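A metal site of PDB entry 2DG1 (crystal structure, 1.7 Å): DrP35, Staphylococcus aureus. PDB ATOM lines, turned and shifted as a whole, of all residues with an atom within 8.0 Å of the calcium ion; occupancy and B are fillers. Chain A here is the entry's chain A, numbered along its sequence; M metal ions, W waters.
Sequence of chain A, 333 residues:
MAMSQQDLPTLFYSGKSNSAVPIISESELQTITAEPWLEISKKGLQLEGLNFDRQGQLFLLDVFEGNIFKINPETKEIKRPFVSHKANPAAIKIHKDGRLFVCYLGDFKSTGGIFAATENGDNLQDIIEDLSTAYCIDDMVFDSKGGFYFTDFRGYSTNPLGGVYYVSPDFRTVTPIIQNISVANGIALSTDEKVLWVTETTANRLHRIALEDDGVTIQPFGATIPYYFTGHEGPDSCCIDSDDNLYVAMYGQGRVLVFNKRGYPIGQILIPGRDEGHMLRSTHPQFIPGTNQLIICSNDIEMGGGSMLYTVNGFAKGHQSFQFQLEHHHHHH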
ATOM      1  N   LEU A  47     -22.420 -18.795 -12.486  1.00  0.00           N
ATOM      2  CA  LEU A  47     -21.120 -18.344 -11.995  1.00  0.00           C
ATOM      3  C   LEU A  47     -19.976 -19.271 -12.407  1.00  0.00           C
ATOM      4  O   LEU A  47     -20.129 -20.490 -12.425  1.00  0.00           O
ATOM      5  CB  LEU A  47     -21.139 -18.201 -10.479  1.00  0.00           C
ATOM      6  CG  LEU A  47     -22.176 -17.256  -9.870  1.00  0.00           C
ATOM      7  CD1 LEU A  47     -21.967 -17.148  -8.369  1.00  0.00           C
ATOM      8  CD2 LEU A  47     -22.078 -15.891 -10.522  1.00  0.00           C
ATOM      9  N   GLU A  48     -18.832 -18.674 -12.714  1.00  0.00           N
ATOM     10  CA  GLU A  48     -17.632 -19.403 -13.121  1.00  0.00           C
ATOM     11  C   GLU A  48     -16.425 -18.469 -13.153  1.00  0.00           C
ATOM     12  O   GLU A  48     -16.560 -17.253 -12.944  1.00  0.00           O
ATOM     13  CB  GLU A  48     -17.828 -19.993 -14.533  1.00  0.00           C
ATOM     14  CG  GLU A  48     -18.020 -21.499 -14.567  1.00  0.00           C
ATOM     15  CD  GLU A  48     -16.715 -22.259 -14.479  1.00  0.00           C
ATOM     16  OE1 GLU A  48     -15.772 -21.791 -13.810  1.00  0.00           O
ATOM     17  OE2 GLU A  48     -16.623 -23.348 -15.086  1.00  0.00           O
ATOM     18  N   GLY A  49     -15.251 -19.043 -13.399  1.00  0.00           N
ATOM     19  CA  GLY A  49     -14.027 -18.278 -13.545  1.00  0.00           C
ATOM     20  C   GLY A  49     -13.395 -17.514 -12.407  1.00  0.00           C
ATOM     21  O   GLY A  49     -12.828 -16.452 -12.626  1.00  0.00           O
ATOM     22  N   VAL A  63     -21.631 -17.262 -17.157  1.00  0.00           N
ATOM     23  CA  VAL A  63     -21.595 -17.697 -18.547  1.00  0.00           C
ATOM     24  C   VAL A  63     -22.626 -17.127 -19.524  1.00  0.00           C
ATOM     25  O   VAL A  63     -22.275 -16.578 -20.569  1.00  0.00           O
ATOM     26  CB  VAL A  63     -21.675 -19.222 -18.628  1.00  0.00           C
ATOM     27  CG1 VAL A  63     -21.430 -19.679 -20.070  1.00  0.00           C
ATOM     28  CG2 VAL A  63     -20.660 -19.845 -17.678  1.00  0.00           C
ATOM     29  N   ALA A  90     -16.282 -18.565 -19.853  1.00  0.00           N
ATOM     30  CA  ALA A  90     -16.338 -19.539 -18.760  1.00  0.00           C
ATOM     31  C   ALA A  90     -15.200 -19.469 -17.740  1.00  0.00           C
ATOM     32  O   ALA A  90     -15.261 -20.139 -16.701  1.00  0.00           O
ATOM     33  CB  ALA A  90     -16.415 -20.946 -19.342  1.00  0.00           C
ATOM     34  N   ALA A  91     -14.168 -18.698 -18.026  1.00  0.00           N
ATOM     35  CA  ALA A  91     -13.055 -18.590 -17.096  1.00  0.00           C
ATOM     36  C   ALA A  91     -12.251 -17.311 -17.245  1.00  0.00           C
ATOM     37  O   ALA A  91     -12.191 -16.711 -18.320  1.00  0.00           O
ATOM     38  CB  ALA A  91     -12.122 -19.800 -17.241  1.00  0.00           C
ATOM     39  N   LYS A  93      -8.388 -15.891 -16.212  1.00  0.00           N
ATOM     40  CA  LYS A  93      -7.059 -16.167 -15.706  1.00  0.00           C
ATOM     41  C   LYS A  93      -6.273 -14.875 -15.893  1.00  0.00           C
ATOM     42  O   LYS A  93      -6.133 -14.397 -17.013  1.00  0.00           O
ATOM     43  CB  LYS A  93      -6.388 -17.313 -16.455  1.00  0.00           C
ATOM     44  CG  LYS A  93      -6.257 -18.597 -15.631  1.00  0.00           C
ATOM     45  CD  LYS A  93      -7.629 -19.157 -15.254  1.00  0.00           C
ATOM     46  CE  LYS A  93      -7.503 -20.303 -14.253  1.00  0.00           C
ATOM     47  NZ  LYS A  93      -8.819 -20.956 -13.991  1.00  0.00           N
ATOM     48  N   LEU A 105     -16.820 -20.062 -24.696  1.00  0.00           N
ATOM     49  CA  LEU A 105     -17.300 -21.192 -25.471  1.00  0.00           C
ATOM     50  C   LEU A 105     -17.999 -20.856 -26.798  1.00  0.00           C
ATOM     51  O   LEU A 105     -18.212 -21.735 -27.628  1.00  0.00           O
ATOM     52  CB  LEU A 105     -18.235 -22.024 -24.602  1.00  0.00           C
ATOM     53  CG  LEU A 105     -17.631 -22.438 -23.251  1.00  0.00           C
ATOM     54  CD1 LEU A 105     -18.688 -23.104 -22.387  1.00  0.00           C
ATOM     55  CD2 LEU A 105     -16.453 -23.371 -23.486  1.00  0.00           C
ATOM     56  N   ASP A 138     -12.865 -23.525 -22.478  1.00  0.00           N
ATOM     57  CA  ASP A 138     -13.477 -23.416 -21.171  1.00  0.00           C
ATOM     58  C   ASP A 138     -12.593 -22.902 -20.035  1.00  0.00           C
ATOM     59  O   ASP A 138     -13.078 -22.227 -19.127  1.00  0.00           O
ATOM     60  CB  ASP A 138     -14.035 -24.772 -20.753  1.00  0.00           C
ATOM     61  CG  ASP A 138     -14.877 -24.697 -19.499  1.00  0.00           C
ATOM     62  OD1 ASP A 138     -16.033 -24.220 -19.604  1.00  0.00           O
ATOM     63  OD2 ASP A 138     -14.381 -25.086 -18.416  1.00  0.00           O
ATOM     64  N   ASP A 139     -11.305 -23.206 -20.086  1.00  0.00           N
ATOM     65  CA  ASP A 139     -10.399 -22.782 -19.025  1.00  0.00           C
ATOM     66  C   ASP A 139      -8.958 -22.805 -19.496  1.00  0.00           C
ATOM     67  O   ASP A 139      -8.656 -23.277 -20.591  1.00  0.00           O
ATOM     68  CB  ASP A 139     -10.564 -23.707 -17.813  1.00  0.00           C
ATOM     69  CG  ASP A 139     -10.301 -23.012 -16.485  1.00  0.00           C
ATOM     70  OD1 ASP A 139      -9.566 -22.008 -16.463  1.00  0.00           O
ATOM     71  OD2 ASP A 139     -10.822 -23.487 -15.449  1.00  0.00           O
ATOM     72  N   MET A 140      -8.058 -22.297 -18.662  1.00  0.00           N
ATOM     73  CA  MET A 140      -6.640 -22.248 -19.009  1.00  0.00           C
ATOM     74  C   MET A 140      -5.817 -22.106 -17.739  1.00  0.00           C
ATOM     75  O   MET A 140      -6.332 -21.850 -16.660  1.00  0.00           O
ATOM     76  CB  MET A 140      -6.368 -21.037 -19.906  1.00  0.00           C
ATOM     77  CG  MET A 140      -6.655 -19.714 -19.189  1.00  0.00           C
ATOM     78  SD  MET A 140      -6.469 -18.248 -20.236  1.00  0.00           S
ATOM     79  CE  MET A 140      -4.679 -18.033 -20.186  1.00  0.00           C
ATOM     80  N   THR A 151      -8.256 -25.761 -22.215  1.00  0.00           N
ATOM     81  CA  THR A 151      -9.135 -26.886 -22.459  1.00  0.00           C
ATOM     82  C   THR A 151     -10.143 -26.614 -23.571  1.00  0.00           C
ATOM     83  O   THR A 151     -10.804 -25.575 -23.581  1.00  0.00           O
ATOM     84  CB  THR A 151      -9.905 -27.286 -21.180  1.00  0.00           C
ATOM     85  OG1 THR A 151     -10.511 -26.124 -20.588  1.00  0.00           O
ATOM     86  CG2 THR A 151      -8.944 -27.929 -20.168  1.00  0.00           C
ATOM     87  N   PHE A 153     -13.436 -27.422 -24.852  1.00  0.00           N
ATOM     88  CA  PHE A 153     -14.725 -27.871 -24.322  1.00  0.00           C
ATOM     89  C   PHE A 153     -15.671 -28.255 -25.457  1.00  0.00           C
ATOM     90  O   PHE A 153     -16.633 -27.521 -25.742  1.00  0.00           O
ATOM     91  CB  PHE A 153     -15.311 -26.707 -23.525  1.00  0.00           C
ATOM     92  CG  PHE A 153     -16.410 -27.084 -22.568  1.00  0.00           C
ATOM     93  CD1 PHE A 153     -16.113 -27.499 -21.273  1.00  0.00           C
ATOM     94  CD2 PHE A 153     -17.743 -26.918 -22.922  1.00  0.00           C
ATOM     95  CE1 PHE A 153     -17.127 -27.742 -20.345  1.00  0.00           C
ATOM     96  CE2 PHE A 153     -18.770 -27.148 -22.007  1.00  0.00           C
ATOM     97  CZ  PHE A 153     -18.460 -27.567 -20.719  1.00  0.00           C
ATOM     98  N   ALA A 184     -13.113 -31.394 -22.464  1.00  0.00           N
ATOM     99  CA  ALA A 184     -12.061 -31.070 -21.505  1.00  0.00           C
ATOM    100  C   ALA A 184     -12.595 -29.851 -20.765  1.00  0.00           C
ATOM    101  O   ALA A 184     -13.115 -28.928 -21.396  1.00  0.00           O
ATOM    102  CB  ALA A 184     -10.760 -30.735 -22.216  1.00  0.00           C
ATOM    103  N   ASN A 185     -12.457 -29.833 -19.451  1.00  0.00           N
ATOM    104  CA  ASN A 185     -13.021 -28.750 -18.661  1.00  0.00           C
ATOM    105  C   ASN A 185     -12.001 -28.101 -17.741  1.00  0.00           C
ATOM    106  O   ASN A 185     -11.455 -27.030 -18.042  1.00  0.00           O
ATOM    107  CB  ASN A 185     -14.188 -29.309 -17.852  1.00  0.00           C
ATOM    108  CG  ASN A 185     -15.048 -28.216 -17.221  1.00  0.00           C
ATOM    109  OD1 ASN A 185     -14.536 -27.186 -16.812  1.00  0.00           O
ATOM    110  ND2 ASN A 185     -16.348 -28.469 -17.128  1.00  0.00           N
ATOM    111  N   GLY A 186     -11.749 -28.742 -16.605  1.00  0.00           N
ATOM    112  CA  GLY A 186     -10.796 -28.185 -15.664  1.00  0.00           C
ATOM    113  C   GLY A 186      -9.368 -28.505 -16.045  1.00  0.00           C
ATOM    114  O   GLY A 186      -9.088 -29.513 -16.692  1.00  0.00           O
ATOM    115  N   ILE A 187      -8.456 -27.634 -15.639  1.00  0.00           N
ATOM    116  CA  ILE A 187      -7.040 -27.847 -15.938  1.00  0.00           C
ATOM    117  C   ILE A 187      -6.198 -27.147 -14.872  1.00  0.00           C
ATOM    118  O   ILE A 187      -6.575 -26.095 -14.351  1.00  0.00           O
ATOM    119  CB  ILE A 187      -6.673 -27.308 -17.339  1.00  0.00           C
ATOM    120  CG1 ILE A 187      -5.252 -27.726 -17.708  1.00  0.00           C
ATOM    121  CG2 ILE A 187      -6.825 -25.789 -17.373  1.00  0.00           C
ATOM    122  CD1 ILE A 187      -4.917 -27.556 -19.171  1.00  0.00           C
ATOM    123  N   THR A 199      -9.785 -32.357 -16.274  1.00  0.00           N
ATOM    124  CA  THR A 199     -11.024 -33.065 -15.981  1.00  0.00           C
ATOM    125  C   THR A 199     -11.819 -33.213 -17.274  1.00  0.00           C
ATOM    126  O   THR A 199     -11.811 -32.329 -18.140  1.00  0.00           O
ATOM    127  CB  THR A 199     -11.882 -32.357 -14.887  1.00  0.00           C
ATOM    128  OG1 THR A 199     -12.371 -31.102 -15.366  1.00  0.00           O
ATOM    129  CG2 THR A 199     -11.046 -32.129 -13.639  1.00  0.00           C
ATOM    130  N   THR A 201     -15.484 -33.802 -18.322  1.00  0.00           N
ATOM    131  CA  THR A 201     -16.850 -33.769 -17.829  1.00  0.00           C
ATOM    132  C   THR A 201     -17.830 -34.840 -18.246  1.00  0.00           C
ATOM    133  O   THR A 201     -18.425 -35.502 -17.395  1.00  0.00           O
ATOM    134  CB  THR A 201     -17.501 -32.409 -18.135  1.00  0.00           C
ATOM    135  OG1 THR A 201     -16.622 -31.358 -17.708  1.00  0.00           O
ATOM    136  CG2 THR A 201     -18.841 -32.264 -17.414  1.00  0.00           C
ATOM    137  N   PRO A 235     -17.046 -33.808 -13.546  1.00  0.00           N
ATOM    138  CA  PRO A 235     -16.077 -32.863 -12.984  1.00  0.00           C
ATOM    139  C   PRO A 235     -16.030 -31.557 -13.777  1.00  0.00           C
ATOM    140  O   PRO A 235     -16.182 -31.558 -14.995  1.00  0.00           O
ATOM    141  CB  PRO A 235     -14.753 -33.625 -13.063  1.00  0.00           C
ATOM    142  CG  PRO A 235     -14.927 -34.434 -14.323  1.00  0.00           C
ATOM    143  CD  PRO A 235     -16.352 -34.950 -14.188  1.00  0.00           C
ATOM    144  N   ASP A 236     -15.797 -30.457 -13.072  1.00  0.00           N
ATOM    145  CA  ASP A 236     -15.727 -29.139 -13.689  1.00  0.00           C
ATOM    146  C   ASP A 236     -14.328 -28.557 -13.474  1.00  0.00           C
ATOM    147  O   ASP A 236     -13.321 -29.264 -13.613  1.00  0.00           O
ATOM    148  CB  ASP A 236     -16.786 -28.213 -13.092  1.00  0.00           C
ATOM    149  CG  ASP A 236     -17.248 -27.135 -14.064  1.00  0.00           C
ATOM    150  OD1 ASP A 236     -16.387 -26.488 -14.704  1.00  0.00           O
ATOM    151  OD2 ASP A 236     -18.470 -26.925 -14.169  1.00  0.00           O
ATOM    152  N   SER A 237     -14.265 -27.280 -13.119  1.00  0.00           N
ATOM    153  CA  SER A 237     -12.994 -26.584 -12.921  1.00  0.00           C
ATOM    154  C   SER A 237     -12.203 -27.047 -11.702  1.00  0.00           C
ATOM    155  O   SER A 237     -12.757 -27.610 -10.761  1.00  0.00           O
ATOM    156  CB  SER A 237     -13.236 -25.087 -12.809  1.00  0.00           C
ATOM    157  OG  SER A 237     -14.232 -24.666 -13.735  1.00  0.00           O
ATOM    158  N   CYS A 238     -10.903 -26.785 -11.728  1.00  0.00           N
ATOM    159  CA  CYS A 238     -10.034 -27.181 -10.630  1.00  0.00           C
ATOM    160  C   CYS A 238      -8.898 -26.202 -10.377  1.00  0.00           C
ATOM    161  O   CYS A 238      -8.587 -25.351 -11.217  1.00  0.00           O
ATOM    162  CB  CYS A 238      -9.470 -28.582 -10.880  1.00  0.00           C
ATOM    163  SG  CYS A 238      -8.557 -28.787 -12.446  1.00  0.00           S
ATOM    164  N   ALA A 249     -14.201 -28.926  -8.645  1.00  0.00           N
ATOM    165  CA  ALA A 249     -15.617 -28.614  -8.469  1.00  0.00           C
ATOM    166  C   ALA A 249     -16.367 -29.640  -9.309  1.00  0.00           C
ATOM    167  O   ALA A 249     -15.984 -29.933 -10.447  1.00  0.00           O
ATOM    168  CB  ALA A 249     -15.908 -27.196  -8.959  1.00  0.00           C
ATOM    169  N   TYR A 251     -19.605 -30.362 -11.262  1.00  0.00           N
ATOM    170  CA  TYR A 251     -20.793 -29.756 -11.847  1.00  0.00           C
ATOM    171  C   TYR A 251     -22.054 -30.603 -11.720  1.00  0.00           C
ATOM    172  O   TYR A 251     -22.083 -31.772 -12.117  1.00  0.00           O
ATOM    173  CB  TYR A 251     -20.552 -29.441 -13.330  1.00  0.00           C
ATOM    174  CG  TYR A 251     -21.663 -28.594 -13.925  1.00  0.00           C
ATOM    175  CD1 TYR A 251     -21.845 -27.276 -13.518  1.00  0.00           C
ATOM    176  CD2 TYR A 251     -22.553 -29.128 -14.859  1.00  0.00           C
ATOM    177  CE1 TYR A 251     -22.891 -26.501 -14.025  1.00  0.00           C
ATOM    178  CE2 TYR A 251     -23.600 -28.359 -15.379  1.00  0.00           C
ATOM    179  CZ  TYR A 251     -23.757 -27.051 -14.952  1.00  0.00           C
ATOM    180  OH  TYR A 251     -24.783 -26.285 -15.464  1.00  0.00           O
ATOM    181  N   SER A 282     -22.040 -26.310  -8.814  1.00  0.00           N
ATOM    182  CA  SER A 282     -20.761 -25.909  -8.232  1.00  0.00           C
ATOM    183  C   SER A 282     -19.760 -26.032  -9.377  1.00  0.00           C
ATOM    184  O   SER A 282     -19.451 -27.129  -9.846  1.00  0.00           O
ATOM    185  CB  SER A 282     -20.389 -26.870  -7.099  1.00  0.00           C
ATOM    186  OG  SER A 282     -20.867 -28.173  -7.393  1.00  0.00           O
ATOM    187  N   THR A 283     -19.226 -24.887  -9.812  1.00  0.00           N
ATOM    188  CA  THR A 283     -18.331 -24.877 -10.963  1.00  0.00           C
ATOM    189  C   THR A 283     -16.850 -24.563 -10.798  1.00  0.00           C
ATOM    190  O   THR A 283     -16.053 -24.979 -11.632  1.00  0.00           O
ATOM    191  CB  THR A 283     -18.836 -23.877 -12.010  1.00  0.00           C
ATOM    192  OG1 THR A 283     -18.869 -22.573 -11.415  1.00  0.00           O
ATOM    193  CG2 THR A 283     -20.222 -24.250 -12.487  1.00  0.00           C
ATOM    194  N   HIS A 284     -16.467 -23.826  -9.764  1.00  0.00           N
ATOM    195  CA  HIS A 284     -15.061 -23.445  -9.660  1.00  0.00           C
ATOM    196  C   HIS A 284     -14.577 -23.193  -8.230  1.00  0.00           C
ATOM    197  O   HIS A 284     -15.305 -22.640  -7.409  1.00  0.00           O
ATOM    198  CB  HIS A 284     -14.856 -22.155 -10.481  1.00  0.00           C
ATOM    199  CG  HIS A 284     -13.519 -22.035 -11.130  1.00  0.00           C
ATOM    200  ND1 HIS A 284     -13.350 -22.093 -12.494  1.00  0.00           N
ATOM    201  CD2 HIS A 284     -12.284 -21.853 -10.607  1.00  0.00           C
ATOM    202  CE1 HIS A 284     -12.073 -21.939 -12.789  1.00  0.00           C
ATOM    203  NE2 HIS A 284     -11.405 -21.789 -11.656  1.00  0.00           N
ATOM    204  N   PRO A 285     -13.347 -23.639  -7.916  1.00  0.00           N
ATOM    205  CA  PRO A 285     -12.741 -23.470  -6.596  1.00  0.00           C
ATOM    206  C   PRO A 285     -11.501 -22.574  -6.754  1.00  0.00           C
ATOM    207  O   PRO A 285     -10.805 -22.642  -7.769  1.00  0.00           O
ATOM    208  CB  PRO A 285     -12.367 -24.885  -6.225  1.00  0.00           C
ATOM    209  CG  PRO A 285     -11.818 -25.406  -7.537  1.00  0.00           C
ATOM    210  CD  PRO A 285     -12.751 -24.802  -8.610  1.00  0.00           C
HETATM  211 CA    CA M   1     -15.030 -25.037 -15.934  1.00  0.00          CA
HETATM  212  O   HOH W   1     -14.269 -22.817 -16.664  1.00  0.00           O
HETATM  213  O   HOH W   2     -17.090 -24.804 -17.305  1.00  0.00           O
HETATM  214  O   HOH W   3     -12.722 -25.395 -15.929  1.00  0.00           O
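The calcium ion is bound by water W3, OD1 of Asp 236, OG of Ser 237, OD1 of Asn 185, water W1, OE2 of Glu 48, water W2 and OD2 of Asp 138. The calcium ion has eight donor atoms within binding distance.
Water W3 bridges the side-chain carboxylate (OD2) of Asp 139 and the backbone carbonyl oxygen (O) of Asn 185.
Of the 29 residues printed, 5 come within 4 Å of the calcium ion. The nearest printed residue that does not touch the calcium ion is Thr 283 (4.4 Å).
N of Asn 185 lies within hydrogen-bond range of O of Thr 199. N of Ser 237 sits close to O of Thr 283, 3.3 Å away. O of Asp 236 is in hydrogen-bond range of OG1 of Thr 199 (2.7 Å). The backbone carbonyl oxygen (O) of Asn 185 lies within hydrogen-bond range of the side-chain hydroxyl (OG1) of Thr 151 (2.9 Å). OG1 of Thr 201 sits at hydrogen-bond distance from ND2 of Asn 185 (3.0 Å). The backbone NH of Asp 138 is in hydrogen-bond range of the backbone carbonyl oxygen of Thr 151, at 3.1 Å. N of Asp 236 is in hydrogen-bond range of O of Ala 249, 2.7 Å away. The side-chain hydroxyl of Ser 237 lies close to a ring nitrogen (ND1) of His 284.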
